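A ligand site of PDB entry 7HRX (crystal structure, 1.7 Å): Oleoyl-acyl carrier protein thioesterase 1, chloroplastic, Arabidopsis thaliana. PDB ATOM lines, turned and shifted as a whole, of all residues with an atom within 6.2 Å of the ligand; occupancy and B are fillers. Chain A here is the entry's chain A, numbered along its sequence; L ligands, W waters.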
ATOM      1  N   GLY A  41     -27.760  20.104   3.545  1.00  0.00           N
ATOM      2  CA  GLY A  41     -26.712  20.453   2.590  1.00  0.00           C
ATOM      3  C   GLY A  41     -25.334  20.384   3.240  1.00  0.00           C
ATOM      4  O   GLY A  41     -24.412  19.799   2.665  1.00  0.00           O
ATOM      5  N   HIS A  44     -24.274  16.810   3.968  1.00  0.00           N
ATOM      6  CA  HIS A  44     -23.851  16.142   2.737  1.00  0.00           C
ATOM      7  C   HIS A  44     -22.381  16.547   2.413  1.00  0.00           C
ATOM      8  O   HIS A  44     -21.566  15.656   2.162  1.00  0.00           O
ATOM      9  CB  HIS A  44     -24.789  16.492   1.552  1.00  0.00           C
ATOM     10  CG  HIS A  44     -24.491  15.732   0.291  1.00  0.00           C
ATOM     11  ND1 HIS A  44     -25.029  16.120  -0.933  1.00  0.00           N
ATOM     12  CD2 HIS A  44     -23.694  14.645   0.092  1.00  0.00           C
ATOM     13  CE1 HIS A  44     -24.555  15.262  -1.824  1.00  0.00           C
ATOM     14  NE2 HIS A  44     -23.726  14.369  -1.254  1.00  0.00           N
ATOM     15  N   ALA A  45     -22.037  17.846   2.523  1.00  0.00           N
ATOM     16  CA  ALA A  45     -20.649  18.310   2.319  1.00  0.00           C
ATOM     17  C   ALA A  45     -19.690  17.595   3.295  1.00  0.00           C
ATOM     18  O   ALA A  45     -18.637  17.081   2.871  1.00  0.00           O
ATOM     19  CB  ALA A  45     -20.545  19.821   2.507  1.00  0.00           C
ATOM     20  N   GLN A  46     -20.070  17.509   4.589  1.00  0.00           N
ATOM     21  CA  GLN A  46     -19.240  16.890   5.614  1.00  0.00           C
ATOM     22  C   GLN A  46     -19.018  15.407   5.301  1.00  0.00           C
ATOM     23  O   GLN A  46     -17.887  14.912   5.395  1.00  0.00           O
ATOM     24  CB  GLN A  46     -19.917  17.043   6.996  1.00  0.00           C
ATOM     25  CG  GLN A  46     -19.007  16.663   8.164  1.00  0.00           C
ATOM     26  CD  GLN A  46     -19.656  17.068   9.460  1.00  0.00           C
ATOM     27  OE1 GLN A  46     -20.095  18.221   9.651  1.00  0.00           O
ATOM     28  NE2 GLN A  46     -19.721  16.120  10.421  1.00  0.00           N
ATOM     29  N   SER A  47     -20.095  14.711   4.915  1.00  0.00           N
ATOM     30  CA  SER A  47     -20.045  13.278   4.606  1.00  0.00           C
ATOM     31  C   SER A  47     -18.991  12.920   3.561  1.00  0.00           C
ATOM     32  O   SER A  47     -18.501  11.796   3.578  1.00  0.00           O
ATOM     33  CB  SER A  47     -21.422  12.758   4.191  1.00  0.00           C
ATOM     34  OG  SER A  47     -21.710  12.986   2.826  1.00  0.00           O
ATOM     35  N   VAL A  48     -18.652  13.842   2.651  1.00  0.00           N
ATOM     36  CA  VAL A  48     -17.657  13.538   1.606  1.00  0.00           C
ATOM     37  C   VAL A  48     -16.344  14.384   1.704  1.00  0.00           C
ATOM     38  O   VAL A  48     -15.540  14.347   0.761  1.00  0.00           O
ATOM     39  CB  VAL A  48     -18.244  13.557   0.175  1.00  0.00           C
ATOM     40  CG1 VAL A  48     -19.287  12.455  -0.018  1.00  0.00           C
ATOM     41  CG2 VAL A  48     -18.828  14.914  -0.161  1.00  0.00           C
ATOM     42  N   PHE A  50     -15.821  17.920   2.347  1.00  0.00           N
ATOM     43  CA  PHE A  50     -15.749  19.343   2.010  1.00  0.00           C
ATOM     44  C   PHE A  50     -15.847  20.219   3.276  1.00  0.00           C
ATOM     45  O   PHE A  50     -16.203  19.695   4.333  1.00  0.00           O
ATOM     46  CB  PHE A  50     -16.877  19.710   1.032  1.00  0.00           C
ATOM     47  CG  PHE A  50     -16.652  19.195  -0.351  1.00  0.00           C
ATOM     48  CD1 PHE A  50     -15.805  19.844  -1.225  1.00  0.00           C
ATOM     49  CD2 PHE A  50     -17.271  18.036  -0.779  1.00  0.00           C
ATOM     50  CE1 PHE A  50     -15.598  19.355  -2.508  1.00  0.00           C
ATOM     51  CE2 PHE A  50     -17.065  17.561  -2.063  1.00  0.00           C
ATOM     52  CZ  PHE A  50     -16.224  18.218  -2.918  1.00  0.00           C
ATOM     53  N   PHE A  55     -19.474  27.390   2.560  1.00  0.00           N
ATOM     54  CA  PHE A  55     -18.776  27.706   1.320  1.00  0.00           C
ATOM     55  C   PHE A  55     -18.309  26.457   0.533  1.00  0.00           C
ATOM     56  O   PHE A  55     -17.725  26.621  -0.553  1.00  0.00           O
ATOM     57  CB  PHE A  55     -17.609  28.663   1.608  1.00  0.00           C
ATOM     58  CG  PHE A  55     -18.017  29.933   2.322  1.00  0.00           C
ATOM     59  CD1 PHE A  55     -19.030  30.744   1.824  1.00  0.00           C
ATOM     60  CD2 PHE A  55     -17.349  30.355   3.463  1.00  0.00           C
ATOM     61  CE1 PHE A  55     -19.381  31.926   2.460  1.00  0.00           C
ATOM     62  CE2 PHE A  55     -17.699  31.538   4.099  1.00  0.00           C
ATOM     63  CZ  PHE A  55     -18.718  32.313   3.604  1.00  0.00           C
ATOM     64  N   ALA A  56     -18.558  25.228   1.066  1.00  0.00           N
ATOM     65  CA  ALA A  56     -18.244  23.931   0.448  1.00  0.00           C
ATOM     66  C   ALA A  56     -16.900  23.909  -0.297  1.00  0.00           C
ATOM     67  O   ALA A  56     -16.830  23.569  -1.473  1.00  0.00           O
ATOM     68  CB  ALA A  56     -19.386  23.540  -0.495  1.00  0.00           C
ATOM     69  N   TRP A  68     -17.807  29.129  -2.502  1.00  0.00           N
ATOM     70  CA  TRP A  68     -19.052  29.000  -3.256  1.00  0.00           C
ATOM     71  C   TRP A  68     -20.073  29.880  -2.534  1.00  0.00           C
ATOM     72  O   TRP A  68     -20.132  29.862  -1.298  1.00  0.00           O
ATOM     73  CB  TRP A  68     -19.549  27.551  -3.271  1.00  0.00           C
ATOM     74  CG  TRP A  68     -18.768  26.643  -4.162  1.00  0.00           C
ATOM     75  CD1 TRP A  68     -17.887  25.671  -3.789  1.00  0.00           C
ATOM     76  CD2 TRP A  68     -18.828  26.602  -5.590  1.00  0.00           C
ATOM     77  NE1 TRP A  68     -17.376  25.042  -4.906  1.00  0.00           N
ATOM     78  CE2 TRP A  68     -17.944  25.590  -6.028  1.00  0.00           C
ATOM     79  CE3 TRP A  68     -19.519  27.358  -6.559  1.00  0.00           C
ATOM     80  CZ2 TRP A  68     -17.776  25.281  -7.370  1.00  0.00           C
ATOM     81  CZ3 TRP A  68     -19.357  27.043  -7.881  1.00  0.00           C
ATOM     82  CH2 TRP A  68     -18.479  26.026  -8.278  1.00  0.00           C
ATOM     83  N   TRP A  92     -28.978  16.698  -3.374  1.00  0.00           N
ATOM     84  CA  TRP A  92     -27.904  16.349  -4.279  1.00  0.00           C
ATOM     85  C   TRP A  92     -27.351  17.613  -4.947  1.00  0.00           C
ATOM     86  O   TRP A  92     -28.000  18.666  -4.973  1.00  0.00           O
ATOM     87  CB  TRP A  92     -28.295  15.252  -5.281  1.00  0.00           C
ATOM     88  CG  TRP A  92     -29.335  15.687  -6.267  1.00  0.00           C
ATOM     89  CD1 TRP A  92     -29.115  16.251  -7.492  1.00  0.00           C
ATOM     90  CD2 TRP A  92     -30.757  15.659  -6.088  1.00  0.00           C
ATOM     91  NE1 TRP A  92     -30.316  16.544  -8.092  1.00  0.00           N
ATOM     92  CE2 TRP A  92     -31.341  16.205  -7.239  1.00  0.00           C
ATOM     93  CE3 TRP A  92     -31.599  15.211  -5.055  1.00  0.00           C
ATOM     94  CZ2 TRP A  92     -32.726  16.286  -7.418  1.00  0.00           C
ATOM     95  CZ3 TRP A  92     -32.970  15.249  -5.252  1.00  0.00           C
ATOM     96  CH2 TRP A  92     -33.519  15.832  -6.397  1.00  0.00           C
ATOM     97  N   CYS A  93     -26.157  17.504  -5.460  1.00  0.00           N
ATOM     98  CA  CYS A  93     -25.483  18.604  -6.124  1.00  0.00           C
ATOM     99  C   CYS A  93     -25.247  18.234  -7.595  1.00  0.00           C
ATOM    100  O   CYS A  93     -25.059  17.055  -7.905  1.00  0.00           O
ATOM    101  CB  CYS A  93     -24.173  18.878  -5.381  1.00  0.00           C
ATOM    102  SG  CYS A  93     -23.113  20.118  -6.138  1.00  0.00           S
ATOM    103  N   THR A 101     -23.091  25.944 -10.171  1.00  0.00           N
ATOM    104  CA  THR A 101     -23.598  24.622  -9.812  1.00  0.00           C
ATOM    105  C   THR A 101     -24.911  24.753  -9.065  1.00  0.00           C
ATOM    106  O   THR A 101     -25.214  25.793  -8.472  1.00  0.00           O
ATOM    107  CB  THR A 101     -22.536  23.690  -9.129  1.00  0.00           C
ATOM    108  OG1 THR A 101     -22.962  23.196  -7.859  1.00  0.00           O
ATOM    109  CG2 THR A 101     -21.182  24.285  -8.998  1.00  0.00           C
ATOM    110  N   ARG A 102     -25.686  23.680  -9.091  1.00  0.00           N
ATOM    111  CA  ARG A 102     -26.995  23.604  -8.482  1.00  0.00           C
ATOM    112  C   ARG A 102     -27.021  22.613  -7.299  1.00  0.00           C
ATOM    113  O   ARG A 102     -26.331  21.574  -7.316  1.00  0.00           O
ATOM    114  CB  ARG A 102     -27.977  23.121  -9.556  1.00  0.00           C
ATOM    115  CG  ARG A 102     -29.373  23.685  -9.473  1.00  0.00           C
ATOM    116  CD  ARG A 102     -30.255  23.162 -10.589  1.00  0.00           C
ATOM    117  NE  ARG A 102     -30.511  21.741 -10.425  1.00  0.00           N
ATOM    118  CZ  ARG A 102     -29.932  20.778 -11.134  1.00  0.00           C
ATOM    119  NH1 ARG A 102     -30.213  19.509 -10.897  1.00  0.00           N
ATOM    120  NH2 ARG A 102     -29.066  21.075 -12.099  1.00  0.00           N
ATOM    121  N   ARG A 103     -27.776  22.929  -6.245  1.00  0.00           N
ATOM    122  CA  ARG A 103     -28.042  21.971  -5.175  1.00  0.00           C
ATOM    123  C   ARG A 103     -29.561  21.924  -5.121  1.00  0.00           C
ATOM    124  O   ARG A 103     -30.194  22.996  -5.078  1.00  0.00           O
ATOM    125  CB  ARG A 103     -27.447  22.345  -3.818  1.00  0.00           C
ATOM    126  CG  ARG A 103     -27.988  21.442  -2.670  1.00  0.00           C
ATOM    127  CD  ARG A 103     -27.149  21.475  -1.403  1.00  0.00           C
ATOM    128  NE  ARG A 103     -25.788  20.961  -1.588  1.00  0.00           N
ATOM    129  CZ  ARG A 103     -25.449  19.673  -1.446  1.00  0.00           C
ATOM    130  NH1 ARG A 103     -24.186  19.289  -1.635  1.00  0.00           N
ATOM    131  NH2 ARG A 103     -26.358  18.770  -1.125  1.00  0.00           N
ATOM    132  N   SER A 121     -31.339  25.604  -5.786  1.00  0.00           N
ATOM    133  CA  SER A 121     -30.485  26.750  -5.527  1.00  0.00           C
ATOM    134  C   SER A 121     -29.371  26.800  -6.568  1.00  0.00           C
ATOM    135  O   SER A 121     -28.926  25.737  -7.035  1.00  0.00           O
ATOM    136  CB  SER A 121     -29.882  26.660  -4.123  1.00  0.00           C
ATOM    137  OG  SER A 121     -29.061  25.514  -3.989  1.00  0.00           O
ATOM    138  N   TRP A 123     -25.478  28.399  -7.321  1.00  0.00           N
ATOM    139  CA  TRP A 123     -24.284  28.841  -6.624  1.00  0.00           C
ATOM    140  C   TRP A 123     -23.221  29.280  -7.635  1.00  0.00           C
ATOM    141  O   TRP A 123     -23.148  28.766  -8.760  1.00  0.00           O
ATOM    142  CB  TRP A 123     -23.728  27.698  -5.747  1.00  0.00           C
ATOM    143  CG  TRP A 123     -24.659  27.198  -4.677  1.00  0.00           C
ATOM    144  CD1 TRP A 123     -25.782  26.454  -4.859  1.00  0.00           C
ATOM    145  CD2 TRP A 123     -24.475  27.301  -3.257  1.00  0.00           C
ATOM    146  NE1 TRP A 123     -26.361  26.149  -3.644  1.00  0.00           N
ATOM    147  CE2 TRP A 123     -25.560  26.640  -2.643  1.00  0.00           C
ATOM    148  CE3 TRP A 123     -23.496  27.910  -2.450  1.00  0.00           C
ATOM    149  CZ2 TRP A 123     -25.688  26.564  -1.260  1.00  0.00           C
ATOM    150  CZ3 TRP A 123     -23.655  27.860  -1.077  1.00  0.00           C
ATOM    151  CH2 TRP A 123     -24.726  27.184  -0.493  1.00  0.00           C
ATOM    152  N   VAL A 124     -22.411  30.262  -7.244  1.00  0.00           N
ATOM    153  CA  VAL A 124     -21.322  30.747  -8.089  1.00  0.00           C
ATOM    154  C   VAL A 124     -20.040  30.783  -7.251  1.00  0.00           C
ATOM    155  O   VAL A 124     -20.103  30.836  -6.018  1.00  0.00           O
ATOM    156  CB  VAL A 124     -21.643  32.136  -8.699  1.00  0.00           C
ATOM    157  CG1 VAL A 124     -22.766  32.018  -9.729  1.00  0.00           C
ATOM    158  CG2 VAL A 124     -22.016  33.152  -7.610  1.00  0.00           C
ATOM    159  N   TYR A 144     -15.225  17.989  -7.266  1.00  0.00           N
ATOM    160  CA  TYR A 144     -16.566  17.714  -6.764  1.00  0.00           C
ATOM    161  C   TYR A 144     -17.457  16.887  -7.732  1.00  0.00           C
ATOM    162  O   TYR A 144     -18.439  16.307  -7.277  1.00  0.00           O
ATOM    163  CB  TYR A 144     -17.274  18.993  -6.269  1.00  0.00           C
ATOM    164  CG  TYR A 144     -17.745  19.930  -7.358  1.00  0.00           C
ATOM    165  CD1 TYR A 144     -19.045  19.849  -7.841  1.00  0.00           C
ATOM    166  CD2 TYR A 144     -16.939  20.955  -7.821  1.00  0.00           C
ATOM    167  CE1 TYR A 144     -19.508  20.736  -8.817  1.00  0.00           C
ATOM    168  CE2 TYR A 144     -17.395  21.850  -8.788  1.00  0.00           C
ATOM    169  CZ  TYR A 144     -18.687  21.733  -9.290  1.00  0.00           C
ATOM    170  OH  TYR A 144     -19.114  22.571 -10.284  1.00  0.00           O
ATOM    171  N   PHE A 147     -18.864  13.399  -6.818  1.00  0.00           N
ATOM    172  CA  PHE A 147     -19.921  13.294  -5.807  1.00  0.00           C
ATOM    173  C   PHE A 147     -21.317  13.700  -6.385  1.00  0.00           C
ATOM    174  O   PHE A 147     -22.299  13.703  -5.654  1.00  0.00           O
ATOM    175  CB  PHE A 147     -19.587  14.153  -4.577  1.00  0.00           C
ATOM    176  CG  PHE A 147     -18.213  13.886  -4.036  1.00  0.00           C
ATOM    177  CD1 PHE A 147     -17.894  12.657  -3.465  1.00  0.00           C
ATOM    178  CD2 PHE A 147     -17.191  14.811  -4.192  1.00  0.00           C
ATOM    179  CE1 PHE A 147     -16.615  12.403  -2.991  1.00  0.00           C
ATOM    180  CE2 PHE A 147     -15.912  14.558  -3.708  1.00  0.00           C
ATOM    181  CZ  PHE A 147     -15.635  13.342  -3.126  1.00  0.00           C
ATOM    182  N   CYS A 148     -21.401  13.990  -7.692  1.00  0.00           N
ATOM    183  CA  CYS A 148     -22.624  14.435  -8.341  1.00  0.00           C
ATOM    184  C   CYS A 148     -23.091  13.405  -9.374  1.00  0.00           C
ATOM    185  O   CYS A 148     -22.262  12.761 -10.021  1.00  0.00           O
ATOM    186  CB  CYS A 148     -22.394  15.792  -8.991  1.00  0.00           C
ATOM    187  SG  CYS A 148     -21.764  17.076  -7.869  1.00  0.00           S
HETATM  188  N1  LIG L   1     -20.429  21.043  -2.913  1.00  0.00           N
HETATM  189  C1  LIG L   1     -20.445  23.269  -4.778  1.00  0.00           C
HETATM  190  C2  LIG L   1     -21.562  22.842  -4.015  1.00  0.00           C
HETATM  191  C3  LIG L   1     -21.576  21.728  -3.017  1.00  0.00           C
HETATM  192  C4  LIG L   1     -20.157  20.125  -1.817  1.00  0.00           C
HETATM  193  C5  LIG L   1     -20.771  18.783  -1.974  1.00  0.00           C
HETATM  194  C6  LIG L   1     -21.617  16.745  -1.830  1.00  0.00           C
HETATM  195  C7  LIG L   1     -24.053  23.717  -4.036  1.00  0.00           C
HETATM  196  C8  LIG L   1     -22.619  23.622  -4.399  1.00  0.00           C
HETATM  197  O1  LIG L   1     -22.203  24.493  -5.370  1.00  0.00           O
HETATM  198  C9  LIG L   1     -20.863  24.268  -5.571  1.00  0.00           C
HETATM  199  O2  LIG L   1     -22.556  21.495  -2.322  1.00  0.00           O
HETATM  200  C10 LIG L   1     -21.094  17.833  -1.093  1.00  0.00           C
HETATM  201  C11 LIG L   1     -21.576  17.112  -3.147  1.00  0.00           C
HETATM  202  O3  LIG L   1     -21.062  18.371  -3.252  1.00  0.00           O
HETATM  203  O   HOH W   1     -17.398  22.008  -3.764  1.00  0.00           O
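N of Phe 50 lies within hydrogen-bond range of O of Ala 45 (3.0 Å).
O of His 44 sits at hydrogen-bond distance from OG of Ser 47, 2.8 Å away.
The backbone carbonyl oxygen (O) of Phe 55 sits at hydrogen-bond distance from the backbone NH (N) of Trp 68.
O of Cys 93 sits close to SG of Cys 148.
The backbone NH of Ser 121 sits at hydrogen-bond distance from the backbone carbonyl oxygen of Arg 103, 2.9 Å away.
The indole nitrogen (NE1) of Trp 123 sits at hydrogen-bond distance from the side-chain hydroxyl (OG) of Ser 121 (2.8 Å).
SG of Cys 93 sits close to O of Arg 102 (3.7 Å).
A ring nitrogen (ND1) of His 44 sits at hydrogen-bond distance from the guanidinium group (NH2) of Arg 103 (3.0 Å).
Water W1 lies within hydrogen-bond range of the backbone carbonyl oxygen (O) of Ala 56 (2.8 Å), the indole nitrogen (NE1) of Trp 68 (3.2 Å) and a nitrogen (N1) of the ligand (3.3 Å).
Residues that only touch the ligand: Trp 68, His 44, Trp 123, Ala 45, Ala 56, Phe 50, Val 48, Cys 93 and Phe 147.
Hydrophobic or aromatic side chains that line the ligand: His 44, Val 48, Phe 50, Ala 56, Trp 68, Trp 123 and Phe 147.
11 residues have an atom within 4 Å of the ligand: His 44, Ala 45, Val 48, Phe 50, Ala 56, Trp 68, Cys 93, Thr 101, Arg 103, Trp 123 and Phe 147.
O1 of the ligand is in hydrogen-bond range of OG1 of Thr 101.
The guanidinium group (NH1) of Arg 103 sits at hydrogen-bond distance from an oxygen (O2) of the ligand (2.8 Å).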
